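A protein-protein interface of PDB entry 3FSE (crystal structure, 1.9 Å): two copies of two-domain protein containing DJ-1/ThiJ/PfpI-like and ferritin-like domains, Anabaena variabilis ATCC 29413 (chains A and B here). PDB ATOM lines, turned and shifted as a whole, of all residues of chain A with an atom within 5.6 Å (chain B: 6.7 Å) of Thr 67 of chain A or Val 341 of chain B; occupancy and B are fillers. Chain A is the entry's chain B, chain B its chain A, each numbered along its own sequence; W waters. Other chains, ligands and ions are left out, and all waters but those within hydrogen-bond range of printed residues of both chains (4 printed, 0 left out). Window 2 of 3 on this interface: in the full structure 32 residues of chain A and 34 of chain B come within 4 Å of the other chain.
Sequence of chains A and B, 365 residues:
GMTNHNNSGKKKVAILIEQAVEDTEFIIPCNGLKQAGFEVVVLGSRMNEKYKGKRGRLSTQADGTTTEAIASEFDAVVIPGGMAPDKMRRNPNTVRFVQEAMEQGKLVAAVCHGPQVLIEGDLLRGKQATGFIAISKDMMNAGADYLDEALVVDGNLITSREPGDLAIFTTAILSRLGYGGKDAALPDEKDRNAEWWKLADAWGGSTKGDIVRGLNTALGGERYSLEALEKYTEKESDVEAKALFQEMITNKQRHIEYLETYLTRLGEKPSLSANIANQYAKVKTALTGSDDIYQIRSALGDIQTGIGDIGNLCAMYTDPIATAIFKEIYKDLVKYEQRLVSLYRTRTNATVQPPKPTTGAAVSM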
ATOM      1  N   GLY A  44      15.267 -10.557  -2.595  1.00  0.00           N
ATOM      2  CA  GLY A  44      13.837 -10.245  -2.675  1.00  0.00           C
ATOM      3  C   GLY A  44      13.359  -9.679  -1.355  1.00  0.00           C
ATOM      4  O   GLY A  44      14.173  -9.286  -0.502  1.00  0.00           O
ATOM      5  N   SER A  45      12.040  -9.587  -1.214  1.00  0.00           N
ATOM      6  CA  SER A  45      11.381  -9.162   0.026  1.00  0.00           C
ATOM      7  C   SER A  45      11.161 -10.352   0.983  1.00  0.00           C
ATOM      8  O   SER A  45      11.083 -10.187   2.208  1.00  0.00           O
ATOM      9  CB  SER A  45      10.048  -8.458  -0.279  1.00  0.00           C
ATOM     10  OG  SER A  45      10.272  -7.225  -0.958  1.00  0.00           O
ATOM     11  N   THR A  65      17.129 -12.051   1.382  1.00  0.00           N
ATOM     12  CA  THR A  65      16.215 -10.959   1.568  1.00  0.00           C
ATOM     13  C   THR A  65      16.967  -9.691   1.933  1.00  0.00           C
ATOM     14  O   THR A  65      18.047  -9.734   2.527  1.00  0.00           O
ATOM     15  CB  THR A  65      15.197 -11.453   2.665  1.00  0.00           C
ATOM     16  OG1 THR A  65      14.086 -12.115   2.044  1.00  0.00           O
ATOM     17  CG2 THR A  65      14.732 -10.401   3.545  1.00  0.00           C
ATOM     18  N   THR A  66      16.402  -8.535   1.585  1.00  0.00           N
ATOM     19  CA  THR A  66      17.010  -7.242   1.969  1.00  0.00           C
ATOM     20  C   THR A  66      16.924  -6.938   3.484  1.00  0.00           C
ATOM     21  O   THR A  66      17.531  -5.983   3.944  1.00  0.00           O
ATOM     22  CB  THR A  66      16.364  -6.093   1.229  1.00  0.00           C
ATOM     23  OG1 THR A  66      14.952  -6.186   1.442  1.00  0.00           O
ATOM     24  CG2 THR A  66      16.708  -6.169  -0.272  1.00  0.00           C
ATOM     25  N   THR A  67      16.112  -7.690   4.222  1.00  0.00           N
ATOM     26  CA  THR A  67      16.015  -7.604   5.692  1.00  0.00           C
ATOM     27  C   THR A  67      17.315  -8.034   6.373  1.00  0.00           C
ATOM     28  O   THR A  67      17.850  -7.288   7.179  1.00  0.00           O
ATOM     29  CB  THR A  67      14.816  -8.405   6.205  1.00  0.00           C
ATOM     30  OG1 THR A  67      13.636  -7.933   5.526  1.00  0.00           O
ATOM     31  CG2 THR A  67      14.636  -8.282   7.727  1.00  0.00           C
ATOM     32  N   GLU A  68      17.822  -9.217   6.041  1.00  0.00           N
ATOM     33  CA  GLU A  68      19.065  -9.707   6.653  1.00  0.00           C
ATOM     34  C   GLU A  68      20.325  -9.440   5.837  1.00  0.00           C
ATOM     35  O   GLU A  68      21.403  -9.662   6.368  1.00  0.00           O
ATOM     36  CB  GLU A  68      19.007 -11.206   7.012  1.00  0.00           C
ATOM     37  CG  GLU A  68      19.252 -12.232   5.862  1.00  0.00           C
ATOM     38  CD  GLU A  68      18.142 -12.310   4.859  1.00  0.00           C
ATOM     39  OE1 GLU A  68      17.090 -11.673   5.076  1.00  0.00           O
ATOM     40  OE2 GLU A  68      18.310 -13.042   3.860  1.00  0.00           O
ATOM     41  N   ALA A  69      20.218  -9.022   4.568  1.00  0.00           N
ATOM     42  CA  ALA A  69      21.420  -8.793   3.738  1.00  0.00           C
ATOM     43  C   ALA A  69      22.323  -7.725   4.353  1.00  0.00           C
ATOM     44  O   ALA A  69      21.836  -6.736   4.904  1.00  0.00           O
ATOM     45  CB  ALA A  69      21.070  -8.440   2.293  1.00  0.00           C
ATOM     46  N   ASN A  91       9.358  -1.322   0.699  1.00  0.00           N
ATOM     47  CA  ASN A  91      10.110  -2.155   1.632  1.00  0.00           C
ATOM     48  C   ASN A  91      11.221  -1.305   2.257  1.00  0.00           C
ATOM     49  O   ASN A  91      12.238  -1.015   1.583  1.00  0.00           O
ATOM     50  CB  ASN A  91      10.685  -3.413   0.935  1.00  0.00           C
ATOM     51  CG  ASN A  91      11.298  -4.414   1.909  1.00  0.00           C
ATOM     52  OD1 ASN A  91      11.845  -4.047   2.937  1.00  0.00           O
ATOM     53  ND2 ASN A  91      11.208  -5.696   1.575  1.00  0.00           N
ATOM     54  N   ASN A  93      13.530  -2.096   4.337  1.00  0.00           N
ATOM     55  CA  ASN A  93      14.804  -2.838   4.352  1.00  0.00           C
ATOM     56  C   ASN A  93      15.544  -2.675   3.015  1.00  0.00           C
ATOM     57  O   ASN A  93      16.763  -2.524   2.996  1.00  0.00           O
ATOM     58  CB  ASN A  93      14.560  -4.321   4.586  1.00  0.00           C
ATOM     59  CG  ASN A  93      13.698  -4.597   5.798  1.00  0.00           C
ATOM     60  OD1 ASN A  93      14.166  -4.461   6.927  1.00  0.00           O
ATOM     61  ND2 ASN A  93      12.429  -4.983   5.571  1.00  0.00           N
ATOM     62  N   ARG A  96      16.812   0.868   2.860  1.00  0.00           N
ATOM     63  CA  ARG A  96      17.963   0.902   3.795  1.00  0.00           C
ATOM     64  C   ARG A  96      19.199   0.255   3.173  1.00  0.00           C
ATOM     65  O   ARG A  96      20.284   0.802   3.228  1.00  0.00           O
ATOM     66  CB  ARG A  96      17.617   0.135   5.084  1.00  0.00           C
ATOM     67  CG  ARG A  96      18.681   0.150   6.196  1.00  0.00           C
ATOM     68  CD  ARG A  96      18.582  -1.072   7.104  1.00  0.00           C
ATOM     69  NE  ARG A  96      19.309  -2.220   6.532  1.00  0.00           N
ATOM     70  CZ  ARG A  96      18.813  -3.398   6.134  1.00  0.00           C
ATOM     71  NH1 ARG A  96      17.530  -3.741   6.309  1.00  0.00           N
ATOM     72  NH2 ARG A  96      19.661  -4.300   5.609  1.00  0.00           N
ATOM     73  N   LEU B 244      10.411 -10.664  23.328  1.00  0.00           N
ATOM     74  CA  LEU B 244       9.926 -10.113  22.054  1.00  0.00           C
ATOM     75  C   LEU B 244       8.783 -10.959  21.530  1.00  0.00           C
ATOM     76  O   LEU B 244       7.753 -10.415  21.173  1.00  0.00           O
ATOM     77  CB  LEU B 244      11.037  -9.996  21.010  1.00  0.00           C
ATOM     78  CG  LEU B 244      10.715  -9.460  19.620  1.00  0.00           C
ATOM     79  CD1 LEU B 244       9.911  -8.171  19.672  1.00  0.00           C
ATOM     80  CD2 LEU B 244      12.029  -9.271  18.846  1.00  0.00           C
ATOM     81  N   ILE B 296      14.465 -17.006  15.983  1.00  0.00           N
ATOM     82  CA  ILE B 296      14.446 -15.617  15.516  1.00  0.00           C
ATOM     83  C   ILE B 296      14.425 -15.634  13.997  1.00  0.00           C
ATOM     84  O   ILE B 296      13.660 -14.901  13.387  1.00  0.00           O
ATOM     85  CB  ILE B 296      15.699 -14.812  15.988  1.00  0.00           C
ATOM     86  CG1 ILE B 296      15.730 -14.672  17.515  1.00  0.00           C
ATOM     87  CG2 ILE B 296      15.736 -13.410  15.313  1.00  0.00           C
ATOM     88  CD1 ILE B 296      17.055 -14.100  18.052  1.00  0.00           C
ATOM     89  N   LEU B 300      11.240 -14.368  11.784  1.00  0.00           N
ATOM     90  CA  LEU B 300      11.523 -13.391  10.719  1.00  0.00           C
ATOM     91  C   LEU B 300      10.912 -13.877   9.401  1.00  0.00           C
ATOM     92  O   LEU B 300      10.207 -13.116   8.732  1.00  0.00           O
ATOM     93  CB  LEU B 300      13.044 -13.132  10.625  1.00  0.00           C
ATOM     94  CG  LEU B 300      13.663 -11.770  10.316  1.00  0.00           C
ATOM     95  CD1 LEU B 300      12.865 -10.586  10.810  1.00  0.00           C
ATOM     96  CD2 LEU B 300      15.091 -11.746  10.914  1.00  0.00           C
ATOM     97  N   GLN B 304       7.858 -12.013   7.328  1.00  0.00           N
ATOM     98  CA  GLN B 304       8.039 -11.617   5.922  1.00  0.00           C
ATOM     99  C   GLN B 304       6.907 -12.160   5.049  1.00  0.00           C
ATOM    100  O   GLN B 304       6.445 -11.464   4.147  1.00  0.00           O
ATOM    101  CB  GLN B 304       9.406 -12.036   5.413  1.00  0.00           C
ATOM    102  CG  GLN B 304      10.492 -11.201   6.069  1.00  0.00           C
ATOM    103  CD  GLN B 304      11.872 -11.695   5.837  1.00  0.00           C
ATOM    104  OE1 GLN B 304      12.103 -12.645   5.084  1.00  0.00           O
ATOM    105  NE2 GLN B 304      12.824 -11.067   6.511  1.00  0.00           N
ATOM    106  N   ILE B 307       3.913  -9.912   5.947  1.00  0.00           N
ATOM    107  CA  ILE B 307       4.079  -8.616   5.270  1.00  0.00           C
ATOM    108  C   ILE B 307       3.648  -8.666   3.795  1.00  0.00           C
ATOM    109  O   ILE B 307       2.952  -7.750   3.314  1.00  0.00           O
ATOM    110  CB  ILE B 307       5.558  -8.079   5.439  1.00  0.00           C
ATOM    111  CG1 ILE B 307       5.800  -7.635   6.895  1.00  0.00           C
ATOM    112  CG2 ILE B 307       5.823  -6.905   4.495  1.00  0.00           C
ATOM    113  CD1 ILE B 307       7.292  -7.397   7.285  1.00  0.00           C
ATOM    114  N   TYR B 336       7.648  -5.003  13.950  1.00  0.00           N
ATOM    115  CA  TYR B 336       8.253  -6.187  14.595  1.00  0.00           C
ATOM    116  C   TYR B 336       9.383  -6.802  13.793  1.00  0.00           C
ATOM    117  O   TYR B 336      10.304  -7.363  14.398  1.00  0.00           O
ATOM    118  CB  TYR B 336       7.228  -7.243  15.009  1.00  0.00           C
ATOM    119  CG  TYR B 336       6.450  -6.801  16.220  1.00  0.00           C
ATOM    120  CD1 TYR B 336       7.095  -6.617  17.469  1.00  0.00           C
ATOM    121  CD2 TYR B 336       5.085  -6.571  16.155  1.00  0.00           C
ATOM    122  CE1 TYR B 336       6.382  -6.200  18.606  1.00  0.00           C
ATOM    123  CE2 TYR B 336       4.370  -6.158  17.287  1.00  0.00           C
ATOM    124  CZ  TYR B 336       5.009  -5.964  18.493  1.00  0.00           C
ATOM    125  OH  TYR B 336       4.255  -5.556  19.563  1.00  0.00           O
ATOM    126  N   GLU B 337       9.307  -6.733  12.460  1.00  0.00           N
ATOM    127  CA  GLU B 337      10.406  -7.189  11.587  1.00  0.00           C
ATOM    128  C   GLU B 337      11.708  -6.443  11.956  1.00  0.00           C
ATOM    129  O   GLU B 337      12.764  -7.068  12.126  1.00  0.00           O
ATOM    130  CB  GLU B 337      10.077  -6.960  10.099  1.00  0.00           C
ATOM    131  CG  GLU B 337      11.090  -7.604   9.131  1.00  0.00           C
ATOM    132  CD  GLU B 337      10.897  -7.224   7.677  1.00  0.00           C
ATOM    133  OE1 GLU B 337      10.280  -6.185   7.385  1.00  0.00           O
ATOM    134  OE2 GLU B 337      11.405  -7.965   6.830  1.00  0.00           O
ATOM    135  N   GLN B 338      11.623  -5.124  12.111  1.00  0.00           N
ATOM    136  CA  GLN B 338      12.791  -4.339  12.529  1.00  0.00           C
ATOM    137  C   GLN B 338      13.338  -4.731  13.887  1.00  0.00           C
ATOM    138  O   GLN B 338      14.564  -4.819  14.060  1.00  0.00           O
ATOM    139  CB  GLN B 338      12.526  -2.828  12.451  1.00  0.00           C
ATOM    140  CG  GLN B 338      12.344  -2.345  11.016  1.00  0.00           C
ATOM    141  CD  GLN B 338      13.470  -2.840  10.073  1.00  0.00           C
ATOM    142  OE1 GLN B 338      14.645  -2.499  10.255  1.00  0.00           O
ATOM    143  NE2 GLN B 338      13.114  -3.701   9.126  1.00  0.00           N
ATOM    144  N   ARG B 339      12.451  -5.001  14.838  1.00  0.00           N
ATOM    145  CA  ARG B 339      12.899  -5.453  16.156  1.00  0.00           C
ATOM    146  C   ARG B 339      13.566  -6.826  16.115  1.00  0.00           C
ATOM    147  O   ARG B 339      14.613  -7.019  16.740  1.00  0.00           O
ATOM    148  CB  ARG B 339      11.748  -5.428  17.136  1.00  0.00           C
ATOM    149  CG  ARG B 339      11.325  -3.978  17.398  1.00  0.00           C
ATOM    150  CD  ARG B 339      10.295  -3.864  18.439  1.00  0.00           C
ATOM    151  NE  ARG B 339      10.717  -4.494  19.687  1.00  0.00           N
ATOM    152  CZ  ARG B 339       9.984  -4.526  20.787  1.00  0.00           C
ATOM    153  NH1 ARG B 339       8.810  -3.915  20.829  1.00  0.00           N
ATOM    154  NH2 ARG B 339      10.452  -5.155  21.864  1.00  0.00           N
ATOM    155  N   LEU B 340      12.962  -7.757  15.380  1.00  0.00           N
ATOM    156  CA  LEU B 340      13.517  -9.099  15.198  1.00  0.00           C
ATOM    157  C   LEU B 340      14.894  -9.073  14.537  1.00  0.00           C
ATOM    158  O   LEU B 340      15.808  -9.771  14.992  1.00  0.00           O
ATOM    159  CB  LEU B 340      12.562 -10.009  14.397  1.00  0.00           C
ATOM    160  CG  LEU B 340      11.387 -10.696  15.105  1.00  0.00           C
ATOM    161  CD1 LEU B 340      10.298 -11.162  14.132  1.00  0.00           C
ATOM    162  CD2 LEU B 340      11.882 -11.872  15.970  1.00  0.00           C
ATOM    163  N   VAL B 341      15.051  -8.260  13.493  1.00  0.00           N
ATOM    164  CA  VAL B 341      16.320  -8.205  12.742  1.00  0.00           C
ATOM    165  C   VAL B 341      17.446  -7.520  13.531  1.00  0.00           C
ATOM    166  O   VAL B 341      18.588  -7.956  13.437  1.00  0.00           O
ATOM    167  CB  VAL B 341      16.134  -7.682  11.284  1.00  0.00           C
ATOM    168  CG1 VAL B 341      15.982  -6.182  11.239  1.00  0.00           C
ATOM    169  CG2 VAL B 341      17.297  -8.166  10.400  1.00  0.00           C
ATOM    170  N   SER B 342      17.131  -6.486  14.325  1.00  0.00           N
ATOM    171  CA  SER B 342      18.145  -5.828  15.168  1.00  0.00           C
ATOM    172  C   SER B 342      18.674  -6.832  16.197  1.00  0.00           C
ATOM    173  O   SER B 342      19.884  -6.885  16.461  1.00  0.00           O
ATOM    174  CB  SER B 342      17.589  -4.589  15.879  1.00  0.00           C
ATOM    175  OG  SER B 342      16.597  -4.939  16.828  1.00  0.00           O
ATOM    176  N   LEU B 343      17.761  -7.631  16.759  1.00  0.00           N
ATOM    177  CA  LEU B 343      18.111  -8.685  17.719  1.00  0.00           C
ATOM    178  C   LEU B 343      18.940  -9.785  17.030  1.00  0.00           C
ATOM    179  O   LEU B 343      19.985 -10.215  17.566  1.00  0.00           O
ATOM    180  CB  LEU B 343      16.850  -9.267  18.361  1.00  0.00           C
ATOM    181  CG  LEU B 343      17.043 -10.165  19.566  1.00  0.00           C
ATOM    182  CD1 LEU B 343      17.649  -9.360  20.735  1.00  0.00           C
ATOM    183  CD2 LEU B 343      15.696 -10.784  19.956  1.00  0.00           C
ATOM    184  N   TYR B 344      18.482 -10.226  15.855  1.00  0.00           N
ATOM    185  CA  TYR B 344      19.229 -11.188  15.013  1.00  0.00           C
ATOM    186  C   TYR B 344      20.670 -10.716  14.749  1.00  0.00           C
ATOM    187  O   TYR B 344      21.609 -11.514  14.903  1.00  0.00           O
ATOM    188  CB  TYR B 344      18.509 -11.448  13.678  1.00  0.00           C
ATOM    189  CG  TYR B 344      19.272 -12.336  12.707  1.00  0.00           C
ATOM    190  CD1 TYR B 344      19.403 -13.707  12.937  1.00  0.00           C
ATOM    191  CD2 TYR B 344      19.862 -11.802  11.546  1.00  0.00           C
ATOM    192  CE1 TYR B 344      20.119 -14.536  12.039  1.00  0.00           C
ATOM    193  CE2 TYR B 344      20.570 -12.613  10.641  1.00  0.00           C
ATOM    194  CZ  TYR B 344      20.695 -13.978  10.895  1.00  0.00           C
ATOM    195  OH  TYR B 344      21.385 -14.785  10.013  1.00  0.00           O
ATOM    196  N   ARG B 345      20.826  -9.438  14.368  1.00  0.00           N
ATOM    197  CA  ARG B 345      22.161  -8.830  14.134  1.00  0.00           C
ATOM    198  C   ARG B 345      23.060  -8.859  15.373  1.00  0.00           C
ATOM    199  O   ARG B 345      24.219  -9.279  15.285  1.00  0.00           O
ATOM    200  CB  ARG B 345      22.058  -7.402  13.568  1.00  0.00           C
ATOM    201  CG  ARG B 345      21.610  -7.366  12.109  1.00  0.00           C
ATOM    202  CD  ARG B 345      21.721  -5.965  11.511  1.00  0.00           C
ATOM    203  NE  ARG B 345      20.829  -4.961  12.117  1.00  0.00           N
ATOM    204  CZ  ARG B 345      19.682  -4.477  11.605  1.00  0.00           C
ATOM    205  NH1 ARG B 345      19.187  -4.871  10.425  1.00  0.00           N
ATOM    206  NH2 ARG B 345      19.008  -3.554  12.298  1.00  0.00           N
ATOM    207  N   THR B 346      22.516  -8.444  16.514  1.00  0.00           N
ATOM    208  CA  THR B 346      23.231  -8.472  17.802  1.00  0.00           C
ATOM    209  C   THR B 346      23.677  -9.894  18.179  1.00  0.00           C
ATOM    210  O   THR B 346      24.843 -10.101  18.569  1.00  0.00           O
ATOM    211  CB  THR B 346      22.362  -7.885  18.933  1.00  0.00           C
ATOM    212  OG1 THR B 346      21.949  -6.557  18.567  1.00  0.00           O
ATOM    213  CG2 THR B 346      23.123  -7.845  20.262  1.00  0.00           C
HETATM  214  O   HOH W   1      10.155  -7.725   4.263  1.00  0.00           O
HETATM  215  O   HOH W   2       9.362  -5.299   5.021  1.00  0.00           O
HETATM  216  O   HOH W   3      20.767  -6.389   8.043  1.00  0.00           O
HETATM  217  O   HOH W   4       8.147  -9.234   3.267  1.00  0.00           O
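N of Thr 65 of chain A sits at hydrogen-bond distance from OE2 of Glu 68 of chain A (2.9 Å). OE2 of Glu 337 of chain B lies within hydrogen-bond range of NE2 of Gln 304 of chain B, at 3.4 Å. The side-chain hydroxyl (OG1) of Thr 67 of chain A lies within hydrogen-bond range of the side-chain amide nitrogen (ND2) of Asn 93 of chain A, at 3.2 Å. The side-chain amide oxygen (OD1) of Asn 91 of chain A is in hydrogen-bond range of the side-chain amide nitrogen (ND2) of Asn 93 of chain A, at 2.9 Å. O of Gln 338 of chain B is in hydrogen-bond range of OG of Ser 342 of chain B. NH1 of Arg 96 of chain A lies close to OD1 of Asn 93 of chain A (3.5 Å).
Of chain B, only Gln 304 (3.3 Å), Glu 337 (2.6 Å) and Val 341 (3.4 Å) come within 4 Å of Thr 67 of chain A. Printed residues of chain A within 4 Å of Gln 304 of chain B: Ser 45, Thr 65 and Thr 67. Printed residues of chain A within 4 Å of Glu 337 of chain B: Thr 67 and Asn 93. Of the printed residues of chain A, Gln 338 of chain B touches Asn 93 (2.6 Å). Of chain A, only Thr 67 comes within 4 Å of Val 341 of chain B.
Of the 10 printed residues of chain A, 4 touch a printed residue of chain B. Printed residues of chain B that touch a printed residue of chain A: Gln 304, Glu 337, Gln 338 and Val 341. Among the printed residues, 7 pairs touch across the chains.
No position is printed for both chains.
Water W2 lies within hydrogen-bond range of the side-chain carboxylate (OE1) of Glu 337 of chain B, the side-chain amide nitrogen (ND2) of Asn 93 of chain A and the side-chain amide oxygen (OD1) of Asn 91 of chain A. Water W1 bridges OE2 of Glu 337 of chain B (2.9 Å) and O of Ser 45 of chain A (3.3 Å). Water W4 bridges the backbone carbonyl oxygen of Gln 304 of chain B (2.9 Å) and the backbone carbonyl oxygen of Ser 45 of chain A (3.3 Å). Water W3 lies within hydrogen-bond range of the backbone carbonyl oxygen of Thr 67 of chain A (3.2 Å), the guanidinium group of Arg 345 of chain B (3.2 Å), the backbone carbonyl oxygen of Ala 69 of chain A (3.3 Å) and the guanidinium group of Arg 96 of chain A (3.4 Å).
O of Ser 45 of chain A touches OE1 of Gln 304 of chain B (3.9 Å). Thr 65 of chain A touches Gln 304 of chain B. Thr 67 of chain A touches Val 341 of chain B (O to CG2, 3.4 Å).
The side-chain amide nitrogen of Gln 338 of chain B is in hydrogen-bond range of the side-chain amide oxygen of Asn 93 of chain A (2.6 Å). NE2 of Gln 304 of chain B lies close to OG1 of Thr 67 of chain A, 3.4 Å away. The side-chain carboxylate (OE2) of Glu 337 of chain B is in hydrogen-bond range of the side-chain hydroxyl (OG1) of Thr 67 of chain A, 2.6 Å away. OE1 of Glu 337 of chain B sits at hydrogen-bond distance from ND2 of Asn 93 of chain A (3.1 Å).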
